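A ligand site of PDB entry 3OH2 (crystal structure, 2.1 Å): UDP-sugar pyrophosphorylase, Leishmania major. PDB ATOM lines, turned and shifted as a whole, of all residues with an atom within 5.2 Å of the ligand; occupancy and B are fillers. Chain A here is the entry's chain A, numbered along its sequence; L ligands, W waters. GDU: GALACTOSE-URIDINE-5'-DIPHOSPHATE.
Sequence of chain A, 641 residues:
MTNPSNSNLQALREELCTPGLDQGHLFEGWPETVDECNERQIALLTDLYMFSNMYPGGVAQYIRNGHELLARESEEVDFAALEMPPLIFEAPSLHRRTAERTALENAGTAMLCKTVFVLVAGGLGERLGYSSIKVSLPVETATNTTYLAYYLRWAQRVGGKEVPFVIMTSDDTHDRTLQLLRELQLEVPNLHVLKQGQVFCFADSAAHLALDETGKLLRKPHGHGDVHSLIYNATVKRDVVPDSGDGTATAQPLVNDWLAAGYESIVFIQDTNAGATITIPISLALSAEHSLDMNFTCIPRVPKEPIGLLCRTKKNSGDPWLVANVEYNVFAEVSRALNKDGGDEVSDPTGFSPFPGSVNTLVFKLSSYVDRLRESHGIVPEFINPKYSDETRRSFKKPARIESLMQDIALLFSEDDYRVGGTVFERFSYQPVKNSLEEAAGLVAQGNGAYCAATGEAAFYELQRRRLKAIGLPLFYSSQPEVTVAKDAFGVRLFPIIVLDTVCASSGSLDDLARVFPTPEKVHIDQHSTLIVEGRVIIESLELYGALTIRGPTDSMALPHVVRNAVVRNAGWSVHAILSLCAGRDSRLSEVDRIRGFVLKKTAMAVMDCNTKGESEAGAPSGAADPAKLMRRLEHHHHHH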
ATOM      1  N   VAL A 120     -29.875   9.970   1.010  1.00  0.00           N
ATOM      2  CA  VAL A 120     -28.559  10.449   1.362  1.00  0.00           C
ATOM      3  C   VAL A 120     -28.077   9.657   2.565  1.00  0.00           C
ATOM      4  O   VAL A 120     -28.672   9.711   3.644  1.00  0.00           O
ATOM      5  CB  VAL A 120     -28.517  12.015   1.547  1.00  0.00           C
ATOM      6  CG1 VAL A 120     -28.722  12.708   0.203  1.00  0.00           C
ATOM      7  CG2 VAL A 120     -29.554  12.512   2.573  1.00  0.00           C
ATOM      8  N   ALA A 121     -27.004   8.912   2.354  1.00  0.00           N
ATOM      9  CA  ALA A 121     -26.530   7.968   3.361  1.00  0.00           C
ATOM     10  C   ALA A 121     -25.006   7.968   3.370  1.00  0.00           C
ATOM     11  O   ALA A 121     -24.375   6.904   3.391  1.00  0.00           O
ATOM     12  CB  ALA A 121     -27.087   6.578   3.056  1.00  0.00           C
ATOM     13  N   GLY A 122     -24.423   9.166   3.307  1.00  0.00           N
ATOM     14  CA  GLY A 122     -22.980   9.323   3.351  1.00  0.00           C
ATOM     15  C   GLY A 122     -22.496   9.705   4.737  1.00  0.00           C
ATOM     16  O   GLY A 122     -21.304   9.741   5.001  1.00  0.00           O
ATOM     17  N   GLY A 123     -23.435   9.960   5.643  1.00  0.00           N
ATOM     18  CA  GLY A 123     -23.075  10.502   6.943  1.00  0.00           C
ATOM     19  C   GLY A 123     -22.798   9.414   7.954  1.00  0.00           C
ATOM     20  O   GLY A 123     -23.305   8.284   7.846  1.00  0.00           O
ATOM     21  N   LEU A 124     -21.998   9.755   8.951  1.00  0.00           N
ATOM     22  CA  LEU A 124     -21.628   8.811   9.995  1.00  0.00           C
ATOM     23  C   LEU A 124     -22.514   8.863  11.225  1.00  0.00           C
ATOM     24  O   LEU A 124     -22.702   7.856  11.903  1.00  0.00           O
ATOM     25  CB  LEU A 124     -20.178   9.015  10.408  1.00  0.00           C
ATOM     26  CG  LEU A 124     -19.217   8.160   9.594  1.00  0.00           C
ATOM     27  CD1 LEU A 124     -17.887   8.156  10.299  1.00  0.00           C
ATOM     28  CD2 LEU A 124     -19.772   6.751   9.469  1.00  0.00           C
ATOM     29  N   LYS A 134     -25.560   3.650   9.414  1.00  0.00           N
ATOM     30  CA  LYS A 134     -26.902   3.941   9.910  1.00  0.00           C
ATOM     31  C   LYS A 134     -28.006   3.180   9.166  1.00  0.00           C
ATOM     32  O   LYS A 134     -29.035   2.837   9.749  1.00  0.00           O
ATOM     33  CB  LYS A 134     -27.167   5.445   9.830  1.00  0.00           C
ATOM     34  CG  LYS A 134     -26.374   6.315  10.843  1.00  0.00           C
ATOM     35  CD  LYS A 134     -27.203   6.662  12.072  1.00  0.00           C
ATOM     36  CE  LYS A 134     -27.251   8.174  12.348  1.00  0.00           C
ATOM     37  NZ  LYS A 134     -28.513   8.848  11.899  1.00  0.00           N
ATOM     38  N   MET A 168     -26.752   8.140  -2.100  1.00  0.00           N
ATOM     39  CA  MET A 168     -25.468   8.803  -1.970  1.00  0.00           C
ATOM     40  C   MET A 168     -24.703   8.175  -0.823  1.00  0.00           C
ATOM     41  O   MET A 168     -25.189   8.140   0.320  1.00  0.00           O
ATOM     42  CB  MET A 168     -25.629  10.312  -1.724  1.00  0.00           C
ATOM     43  CG  MET A 168     -24.274  11.055  -1.744  1.00  0.00           C
ATOM     44  SD  MET A 168     -24.283  12.874  -1.632  1.00  0.00           S
ATOM     45  CE  MET A 168     -24.898  13.100   0.049  1.00  0.00           C
ATOM     46  N   GLN A 196     -19.965  10.513  -2.634  1.00  0.00           N
ATOM     47  CA  GLN A 196     -19.494  11.891  -2.531  1.00  0.00           C
ATOM     48  C   GLN A 196     -18.005  11.914  -2.225  1.00  0.00           C
ATOM     49  O   GLN A 196     -17.457  10.948  -1.672  1.00  0.00           O
ATOM     50  CB  GLN A 196     -20.284  12.685  -1.479  1.00  0.00           C
ATOM     51  CG  GLN A 196     -20.113  12.197  -0.046  1.00  0.00           C
ATOM     52  CD  GLN A 196     -21.100  12.868   0.915  1.00  0.00           C
ATOM     53  OE1 GLN A 196     -22.001  12.221   1.469  1.00  0.00           O
ATOM     54  NE2 GLN A 196     -20.932  14.169   1.105  1.00  0.00           N
ATOM     55  N   PRO A 221     -16.044  14.488   4.390  1.00  0.00           N
ATOM     56  CA  PRO A 221     -16.967  14.853   3.316  1.00  0.00           C
ATOM     57  C   PRO A 221     -17.527  16.270   3.475  1.00  0.00           C
ATOM     58  O   PRO A 221     -17.352  16.908   4.513  1.00  0.00           O
ATOM     59  CB  PRO A 221     -18.106  13.810   3.455  1.00  0.00           C
ATOM     60  CG  PRO A 221     -17.480  12.684   4.205  1.00  0.00           C
ATOM     61  CD  PRO A 221     -16.524  13.327   5.164  1.00  0.00           C
ATOM     62  N   HIS A 222     -18.205  16.719   2.442  1.00  0.00           N
ATOM     63  CA  HIS A 222     -18.573  18.120   2.253  1.00  0.00           C
ATOM     64  C   HIS A 222     -20.054  18.338   2.586  1.00  0.00           C
ATOM     65  O   HIS A 222     -20.610  19.401   2.325  1.00  0.00           O
ATOM     66  CB  HIS A 222     -18.247  18.459   0.786  1.00  0.00           C
ATOM     67  CG  HIS A 222     -18.508  19.870   0.381  1.00  0.00           C
ATOM     68  ND1 HIS A 222     -19.525  20.221  -0.473  1.00  0.00           N
ATOM     69  CD2 HIS A 222     -17.842  21.017   0.665  1.00  0.00           C
ATOM     70  CE1 HIS A 222     -19.501  21.528  -0.686  1.00  0.00           C
ATOM     71  NE2 HIS A 222     -18.491  22.033  -0.006  1.00  0.00           N
ATOM     72  N   GLY A 223     -20.687  17.315   3.165  1.00  0.00           N
ATOM     73  CA  GLY A 223     -22.054  17.411   3.637  1.00  0.00           C
ATOM     74  C   GLY A 223     -23.086  16.795   2.696  1.00  0.00           C
ATOM     75  O   GLY A 223     -22.750  16.402   1.594  1.00  0.00           O
ATOM     76  N   HIS A 224     -24.343  16.738   3.121  1.00  0.00           N
ATOM     77  CA  HIS A 224     -25.359  16.147   2.284  1.00  0.00           C
ATOM     78  C   HIS A 224     -25.665  17.009   1.064  1.00  0.00           C
ATOM     79  O   HIS A 224     -26.328  16.560   0.130  1.00  0.00           O
ATOM     80  CB  HIS A 224     -26.617  15.740   3.066  1.00  0.00           C
ATOM     81  CG  HIS A 224     -27.098  16.751   4.066  1.00  0.00           C
ATOM     82  ND1 HIS A 224     -27.812  17.880   3.710  1.00  0.00           N
ATOM     83  CD2 HIS A 224     -27.039  16.762   5.421  1.00  0.00           C
ATOM     84  CE1 HIS A 224     -28.120  18.561   4.801  1.00  0.00           C
ATOM     85  NE2 HIS A 224     -27.668  17.905   5.854  1.00  0.00           N
ATOM     86  N   ILE A 269     -34.674  11.670   0.796  1.00  0.00           N
ATOM     87  CA  ILE A 269     -34.926  11.231   2.154  1.00  0.00           C
ATOM     88  C   ILE A 269     -33.614  11.007   2.890  1.00  0.00           C
ATOM     89  O   ILE A 269     -32.578  10.794   2.268  1.00  0.00           O
ATOM     90  CB  ILE A 269     -35.716   9.912   2.175  1.00  0.00           C
ATOM     91  CG1 ILE A 269     -34.960   8.834   1.420  1.00  0.00           C
ATOM     92  CG2 ILE A 269     -37.115  10.129   1.600  1.00  0.00           C
ATOM     93  CD1 ILE A 269     -35.602   7.404   1.603  1.00  0.00           C
ATOM     94  N   GLN A 270     -33.677  11.023   4.222  1.00  0.00           N
ATOM     95  CA  GLN A 270     -32.491  10.809   5.062  1.00  0.00           C
ATOM     96  C   GLN A 270     -32.439   9.390   5.646  1.00  0.00           C
ATOM     97  O   GLN A 270     -33.393   8.594   5.487  1.00  0.00           O
ATOM     98  CB  GLN A 270     -32.404  11.885   6.154  1.00  0.00           C
ATOM     99  CG  GLN A 270     -32.410  13.275   5.509  1.00  0.00           C
ATOM    100  CD  GLN A 270     -31.876  14.382   6.393  1.00  0.00           C
ATOM    101  OE1 GLN A 270     -31.168  15.288   5.917  1.00  0.00           O
ATOM    102  NE2 GLN A 270     -32.217  14.327   7.683  1.00  0.00           N
ATOM    103  N   ASP A 271     -31.327   9.070   6.313  1.00  0.00           N
ATOM    104  CA  ASP A 271     -30.951   7.691   6.538  1.00  0.00           C
ATOM    105  C   ASP A 271     -31.791   6.917   7.584  1.00  0.00           C
ATOM    106  O   ASP A 271     -31.927   5.726   7.446  1.00  0.00           O
ATOM    107  CB  ASP A 271     -29.448   7.527   6.804  1.00  0.00           C
ATOM    108  CG  ASP A 271     -28.935   8.411   7.950  1.00  0.00           C
ATOM    109  OD1 ASP A 271     -29.770   8.903   8.740  1.00  0.00           O
ATOM    110  OD2 ASP A 271     -27.694   8.606   8.051  1.00  0.00           O
ATOM    111  N   THR A 272     -32.338   7.582   8.598  1.00  0.00           N
ATOM    112  CA  THR A 272     -33.046   6.841   9.640  1.00  0.00           C
ATOM    113  C   THR A 272     -34.376   7.447  10.057  1.00  0.00           C
ATOM    114  O   THR A 272     -34.633   7.595  11.243  1.00  0.00           O
ATOM    115  CB  THR A 272     -32.196   6.700  10.929  1.00  0.00           C
ATOM    116  OG1 THR A 272     -31.927   7.999  11.496  1.00  0.00           O
ATOM    117  CG2 THR A 272     -30.902   5.983  10.629  1.00  0.00           C
ATOM    118  N   PRO A 306     -32.708  20.086  16.910  1.00  0.00           N
ATOM    119  CA  PRO A 306     -31.740  20.186  15.818  1.00  0.00           C
ATOM    120  C   PRO A 306     -32.370  19.945  14.464  1.00  0.00           C
ATOM    121  O   PRO A 306     -31.932  19.083  13.694  1.00  0.00           O
ATOM    122  CB  PRO A 306     -30.741  19.059  16.128  1.00  0.00           C
ATOM    123  CG  PRO A 306     -31.133  18.523  17.492  1.00  0.00           C
ATOM    124  CD  PRO A 306     -32.594  18.792  17.601  1.00  0.00           C
ATOM    125  N   ILE A 307     -33.450  20.683  14.181  1.00  0.00           N
ATOM    126  CA  ILE A 307     -33.989  20.735  12.838  1.00  0.00           C
ATOM    127  C   ILE A 307     -34.086  22.218  12.477  1.00  0.00           C
ATOM    128  O   ILE A 307     -34.325  23.062  13.349  1.00  0.00           O
ATOM    129  CB  ILE A 307     -35.367  20.026  12.703  1.00  0.00           C
ATOM    130  CG1 ILE A 307     -36.444  20.738  13.507  1.00  0.00           C
ATOM    131  CG2 ILE A 307     -35.263  18.573  13.154  1.00  0.00           C
ATOM    132  CD1 ILE A 307     -37.837  20.164  13.312  1.00  0.00           C
ATOM    133  N   GLY A 308     -33.880  22.536  11.210  1.00  0.00           N
ATOM    134  CA  GLY A 308     -33.918  23.925  10.767  1.00  0.00           C
ATOM    135  C   GLY A 308     -35.335  24.469  10.721  1.00  0.00           C
ATOM    136  O   GLY A 308     -36.302  23.731  10.935  1.00  0.00           O
ATOM    137  N   ASN A 325     -34.717  27.029   4.270  1.00  0.00           N
ATOM    138  CA  ASN A 325     -34.433  26.539   5.616  1.00  0.00           C
ATOM    139  C   ASN A 325     -33.425  27.515   6.213  1.00  0.00           C
ATOM    140  O   ASN A 325     -32.556  27.988   5.496  1.00  0.00           O
ATOM    141  CB  ASN A 325     -33.836  25.128   5.513  1.00  0.00           C
ATOM    142  CG  ASN A 325     -33.367  24.573   6.857  1.00  0.00           C
ATOM    143  OD1 ASN A 325     -32.169  24.345   7.071  1.00  0.00           O
ATOM    144  ND2 ASN A 325     -34.298  24.325   7.759  1.00  0.00           N
ATOM    145  N   GLU A 327     -30.928  26.917   9.353  1.00  0.00           N
ATOM    146  CA  GLU A 327     -30.566  25.819  10.266  1.00  0.00           C
ATOM    147  C   GLU A 327     -30.695  26.205  11.741  1.00  0.00           C
ATOM    148  O   GLU A 327     -30.555  27.361  12.112  1.00  0.00           O
ATOM    149  CB  GLU A 327     -29.133  25.327  10.034  1.00  0.00           C
ATOM    150  CG  GLU A 327     -28.972  24.152   9.088  1.00  0.00           C
ATOM    151  CD  GLU A 327     -29.818  22.941   9.438  1.00  0.00           C
ATOM    152  OE1 GLU A 327     -31.063  23.055   9.369  1.00  0.00           O
ATOM    153  OE2 GLU A 327     -29.239  21.872   9.717  1.00  0.00           O
ATOM    154  N   TYR A 328     -30.937  25.187  12.569  1.00  0.00           N
ATOM    155  CA  TYR A 328     -31.133  25.382  13.994  1.00  0.00           C
ATOM    156  C   TYR A 328     -29.992  26.164  14.646  1.00  0.00           C
ATOM    157  O   TYR A 328     -30.259  27.104  15.398  1.00  0.00           O
ATOM    158  CB  TYR A 328     -31.345  24.033  14.702  1.00  0.00           C
ATOM    159  CG  TYR A 328     -30.236  23.022  14.463  1.00  0.00           C
ATOM    160  CD1 TYR A 328     -29.178  22.914  15.349  1.00  0.00           C
ATOM    161  CD2 TYR A 328     -30.267  22.169  13.365  1.00  0.00           C
ATOM    162  CE1 TYR A 328     -28.171  21.989  15.155  1.00  0.00           C
ATOM    163  CE2 TYR A 328     -29.247  21.237  13.153  1.00  0.00           C
ATOM    164  CZ  TYR A 328     -28.201  21.172  14.059  1.00  0.00           C
ATOM    165  OH  TYR A 328     -27.186  20.269  13.901  1.00  0.00           O
ATOM    166  N   SER A 358     -38.189  22.020   9.559  1.00  0.00           N
ATOM    167  CA  SER A 358     -37.927  21.267   8.329  1.00  0.00           C
ATOM    168  C   SER A 358     -37.204  19.956   8.621  1.00  0.00           C
ATOM    169  O   SER A 358     -36.115  19.948   9.175  1.00  0.00           O
ATOM    170  CB  SER A 358     -37.082  22.128   7.377  1.00  0.00           C
ATOM    171  OG  SER A 358     -36.699  21.423   6.206  1.00  0.00           O
ATOM    172  N   VAL A 359     -37.779  18.834   8.202  1.00  0.00           N
ATOM    173  CA  VAL A 359     -37.196  17.537   8.530  1.00  0.00           C
ATOM    174  C   VAL A 359     -36.419  16.898   7.377  1.00  0.00           C
ATOM    175  O   VAL A 359     -35.899  15.795   7.515  1.00  0.00           O
ATOM    176  CB  VAL A 359     -38.233  16.544   9.146  1.00  0.00           C
ATOM    177  CG1 VAL A 359     -38.969  17.223  10.317  1.00  0.00           C
ATOM    178  CG2 VAL A 359     -39.238  16.060   8.107  1.00  0.00           C
ATOM    179  N   ASN A 360     -36.281  17.609   6.254  1.00  0.00           N
ATOM    180  CA  ASN A 360     -35.409  17.177   5.152  1.00  0.00           C
ATOM    181  C   ASN A 360     -35.856  15.912   4.437  1.00  0.00           C
ATOM    182  O   ASN A 360     -35.048  15.081   4.017  1.00  0.00           O
ATOM    183  CB  ASN A 360     -33.928  17.060   5.583  1.00  0.00           C
ATOM    184  CG  ASN A 360     -33.058  18.204   5.002  1.00  0.00           C
ATOM    185  OD1 ASN A 360     -31.830  18.097   4.948  1.00  0.00           O
ATOM    186  ND2 ASN A 360     -33.697  19.289   4.596  1.00  0.00           N
ATOM    187  N   LEU A 405     -25.650  21.887   2.680  1.00  0.00           N
ATOM    188  CA  LEU A 405     -26.913  21.247   3.018  1.00  0.00           C
ATOM    189  C   LEU A 405     -27.709  21.033   1.744  1.00  0.00           C
ATOM    190  O   LEU A 405     -27.812  21.937   0.921  1.00  0.00           O
ATOM    191  CB  LEU A 405     -27.712  22.157   3.937  1.00  0.00           C
ATOM    192  CG  LEU A 405     -26.973  22.695   5.161  1.00  0.00           C
ATOM    193  CD1 LEU A 405     -27.807  23.806   5.742  1.00  0.00           C
ATOM    194  CD2 LEU A 405     -26.763  21.577   6.167  1.00  0.00           C
ATOM    195  N   GLN A 407     -30.820  20.844   1.350  1.00  0.00           N
ATOM    196  CA  GLN A 407     -31.992  21.727   1.301  1.00  0.00           C
ATOM    197  C   GLN A 407     -31.688  23.148   0.781  1.00  0.00           C
ATOM    198  O   GLN A 407     -32.600  23.861   0.344  1.00  0.00           O
ATOM    199  CB  GLN A 407     -32.721  21.788   2.662  1.00  0.00           C
ATOM    200  CG  GLN A 407     -31.959  22.447   3.818  1.00  0.00           C
ATOM    201  CD  GLN A 407     -31.136  21.464   4.629  1.00  0.00           C
ATOM    202  OE1 GLN A 407     -30.604  20.493   4.088  1.00  0.00           O
ATOM    203  NE2 GLN A 407     -31.039  21.692   5.939  1.00  0.00           N
ATOM    204  N   TYR A 430     -42.310  12.244  12.457  1.00  0.00           N
ATOM    205  CA  TYR A 430     -40.851  12.445  12.329  1.00  0.00           C
ATOM    206  C   TYR A 430     -40.191  11.561  13.376  1.00  0.00           C
ATOM    207  O   TYR A 430     -40.280  11.858  14.560  1.00  0.00           O
ATOM    208  CB  TYR A 430     -40.501  13.926  12.587  1.00  0.00           C
ATOM    209  CG  TYR A 430     -39.006  14.240  12.682  1.00  0.00           C
ATOM    210  CD1 TYR A 430     -38.141  13.963  11.620  1.00  0.00           C
ATOM    211  CD2 TYR A 430     -38.467  14.843  13.818  1.00  0.00           C
ATOM    212  CE1 TYR A 430     -36.778  14.267  11.710  1.00  0.00           C
ATOM    213  CE2 TYR A 430     -37.116  15.150  13.903  1.00  0.00           C
ATOM    214  CZ  TYR A 430     -36.289  14.851  12.847  1.00  0.00           C
ATOM    215  OH  TYR A 430     -34.944  15.131  12.928  1.00  0.00           O
ATOM    216  N   PRO A 432     -36.673  10.110  13.698  1.00  0.00           N
ATOM    217  CA  PRO A 432     -35.261   9.797  13.408  1.00  0.00           C
ATOM    218  C   PRO A 432     -34.605   8.978  14.512  1.00  0.00           C
ATOM    219  O   PRO A 432     -35.001   9.074  15.687  1.00  0.00           O
ATOM    220  CB  PRO A 432     -34.594  11.183  13.390  1.00  0.00           C
ATOM    221  CG  PRO A 432     -35.452  12.001  14.324  1.00  0.00           C
ATOM    222  CD  PRO A 432     -36.865  11.541  14.023  1.00  0.00           C
ATOM    223  N   LYS A 434     -31.092   9.270  16.018  1.00  0.00           N
ATOM    224  CA  LYS A 434     -29.938  10.185  15.992  1.00  0.00           C
ATOM    225  C   LYS A 434     -29.073  10.141  17.240  1.00  0.00           C
ATOM    226  O   LYS A 434     -27.853  10.295  17.149  1.00  0.00           O
ATOM    227  CB  LYS A 434     -30.425  11.622  15.816  1.00  0.00           C
ATOM    228  CG  LYS A 434     -31.001  11.886  14.466  1.00  0.00           C
ATOM    229  CD  LYS A 434     -30.518  13.201  13.928  1.00  0.00           C
ATOM    230  CE  LYS A 434     -31.126  13.438  12.606  1.00  0.00           C
ATOM    231  NZ  LYS A 434     -30.597  14.679  12.016  1.00  0.00           N
HETATM  232  N1  GDU L   1     -25.224  12.851   5.019  1.00  0.00           N
HETATM  233  C2  GDU L   1     -24.494  12.623   3.805  1.00  0.00           C
HETATM  234  N3  GDU L   1     -23.224  13.188   3.571  1.00  0.00           N
HETATM  235  C4  GDU L   1     -22.727  13.954   4.544  1.00  0.00           C
HETATM  236  C5  GDU L   1     -23.386  14.230   5.786  1.00  0.00           C
HETATM  237  C6  GDU L   1     -24.613  13.662   5.982  1.00  0.00           C
HETATM  238  O2  GDU L   1     -25.076  11.900   2.997  1.00  0.00           O
HETATM  239  O4  GDU L   1     -21.492  14.445   4.270  1.00  0.00           O
HETATM  240  C1D GDU L   1     -26.599  12.318   5.270  1.00  0.00           C
HETATM  241  C2D GDU L   1     -26.772  11.378   6.513  1.00  0.00           C
HETATM  242  O2D GDU L   1     -26.321  10.111   6.219  1.00  0.00           O
HETATM  243  C3D GDU L   1     -28.316  11.524   6.775  1.00  0.00           C
HETATM  244  C4D GDU L   1     -28.375  13.053   6.494  1.00  0.00           C
HETATM  245  O4D GDU L   1     -27.588  13.330   5.339  1.00  0.00           O
HETATM  246  O3D GDU L   1     -29.117  10.662   6.016  1.00  0.00           O
HETATM  247  C5D GDU L   1     -27.493  13.784   7.550  1.00  0.00           C
HETATM  248  O5D GDU L   1     -28.285  14.550   8.344  1.00  0.00           O
HETATM  249  PA  GDU L   1     -27.927  14.506   9.931  1.00  0.00           P
HETATM  250  O1A GDU L   1     -28.842  13.379  10.497  1.00  0.00           O
HETATM  251  O2A GDU L   1     -26.477  14.258  10.245  1.00  0.00           O
HETATM  252  O3A GDU L   1     -28.461  15.817  10.539  1.00  0.00           O
HETATM  253  PB  GDU L   1     -28.322  17.319   9.976  1.00  0.00           P
HETATM  254  O1B GDU L   1     -27.889  17.916  11.350  1.00  0.00           O
HETATM  255  O2B GDU L   1     -27.344  17.210   8.861  1.00  0.00           O
HETATM  256  O3B GDU L   1     -29.724  17.964   9.666  1.00  0.00           O
HETATM  257  C1' GDU L   1     -30.635  17.716   8.636  1.00  0.00           C
HETATM  258  C2' GDU L   1     -31.158  19.109   8.156  1.00  0.00           C
HETATM  259  C3' GDU L   1     -32.033  19.752   9.262  1.00  0.00           C
HETATM  260  C4' GDU L   1     -33.177  18.755   9.648  1.00  0.00           C
HETATM  261  C5' GDU L   1     -32.650  17.338  10.032  1.00  0.00           C
HETATM  262  C6' GDU L   1     -33.834  16.320  10.210  1.00  0.00           C
HETATM  263  O2' GDU L   1     -30.032  19.886   7.864  1.00  0.00           O
HETATM  264  O3' GDU L   1     -32.583  20.981   8.899  1.00  0.00           O
HETATM  265  O4' GDU L   1     -33.943  18.586   8.474  1.00  0.00           O
HETATM  266  O5' GDU L   1     -31.628  16.856   9.172  1.00  0.00           O
HETATM  267  O6' GDU L   1     -33.283  15.110  10.692  1.00  0.00           O
HETATM  268  O   HOH W   1     -20.033  15.371   6.264  1.00  0.00           O
HETATM  269  O   HOH W   2     -25.299  18.948   8.388  1.00  0.00           O
HETATM  270  O   HOH W   3     -34.026  12.818   9.528  1.00  0.00           O
HETATM  271  O   HOH W   4     -25.632   7.323   6.655  1.00  0.00           O
HETATM  272  O   HOH W   5     -24.798  12.244   9.488  1.00  0.00           O
HETATM  273  O   HOH W   6     -34.177  21.293   6.479  1.00  0.00           O
HETATM  274  O   HOH W   7     -30.206  11.104  10.100  1.00  0.00           O
HETATM  275  O   HOH W   8     -29.861  17.129  13.157  1.00  0.00           O
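The backbone NH (N) of Gly 308 lies within hydrogen-bond range of an oxygen (O3') of the ligand. The backbone carbonyl oxygen (O) of Val 120 sits at hydrogen-bond distance from an oxygen (O3D) of the ligand (2.6 Å). The backbone carbonyl oxygen of Ser 358 is in hydrogen-bond range of an oxygen (O4') of the ligand (2.7 Å). O4 of the ligand lies close to N of Gly 223 (3.2 Å). The side-chain carboxylate (OD2) of Asp 271 lies within hydrogen-bond range of an oxygen (O2D) of the ligand (2.7 Å). An oxygen (O2D) of the ligand lies within hydrogen-bond range of the backbone NH (N) of Gly 123 (2.9 Å). An oxygen (O3D) of the ligand sits at hydrogen-bond distance from the backbone NH (N) of Asp 271 (2.7 Å). OH of Tyr 430 is in hydrogen-bond range of O6' of the ligand, 2.8 Å away. O1A of the ligand lies within salt-bridge range of NZ of Lys 434. OE1 of Glu 327 sits at hydrogen-bond distance from O3' of the ligand, 2.6 Å away. NE2 of Gln 270 lies within hydrogen-bond range of O5' of the ligand, 3.0 Å away. The side-chain amide oxygen (OE1) of Gln 196 sits at hydrogen-bond distance from a nitrogen (N3) of the ligand. NE2 of His 224 lies within hydrogen-bond range of O2B of the ligand (3.1 Å). O4' of the ligand lies close to N of Asn 360 (3.4 Å). O2' of the ligand is in hydrogen-bond range of NE2 of Gln 407, 2.8 Å away. An oxygen (O2) of the ligand lies within hydrogen-bond range of the backbone NH (N) of Gly 122 (2.8 Å).
The side-chain carboxylate (OE1) of Glu 327 lies close to the side-chain amide oxygen (OD1) of Asn 325 (2.9 Å). The side-chain amide nitrogen of Gln 196 sits at hydrogen-bond distance from the backbone carbonyl oxygen of Gly 223 (2.9 Å). The backbone NH (N) of Gly 308 lies close to the side-chain carboxylate (OE1) of Glu 327. NE2 of Gln 407 is in hydrogen-bond range of OD1 of Asn 325. The side-chain amide oxygen (OD1) of Asn 360 sits close to the side-chain amide oxygen (OE1) of Gln 270, 3.0 Å away. N of Gly 122 sits at hydrogen-bond distance from O of Met 168 (3.2 Å). N of Val 120 is in hydrogen-bond range of O of Ile 269, 3.1 Å away. The backbone carbonyl oxygen of Met 168 is in hydrogen-bond range of the backbone NH of Ala 121.
Residues that only touch the ligand: Met 168 (3.2 Å), Val 359 (3.2 Å), Pro 221 (3.5 Å), Tyr 328 (3.5 Å), Ala 121 (3.6 Å), Ile 307 (3.8 Å) and Asn 325 (3.9 Å). Hydrophobic or aromatic side chains within 4 Å of the ligand: Val 120, Met 168, Pro 221, His 224, Ile 307 and Tyr 430.
Water W3 bridges O6' of the ligand (2.7 Å) and NE2 of Gln 270 (3.0 Å). Water W7 lies within hydrogen-bond range of the side-chain carboxylate (OD1) of Asp 271 (2.6 Å), an oxygen (O1A) of the ligand (2.7 Å) and the side-chain amino group (NZ) of Lys 134 (3.3 Å). Water W8 lies within hydrogen-bond range of an oxygen (O1B) of the ligand (2.8 Å), the side-chain amino group of Lys 434 (2.8 Å) and the backbone carbonyl oxygen of Pro 306 (2.9 Å). Water W4 lies within hydrogen-bond range of the backbone carbonyl oxygen (O) of Gly 123 (2.8 Å), the side-chain carboxylate (OD2) of Asp 271 (2.8 Å) and an oxygen (O2D) of the ligand (2.9 Å).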
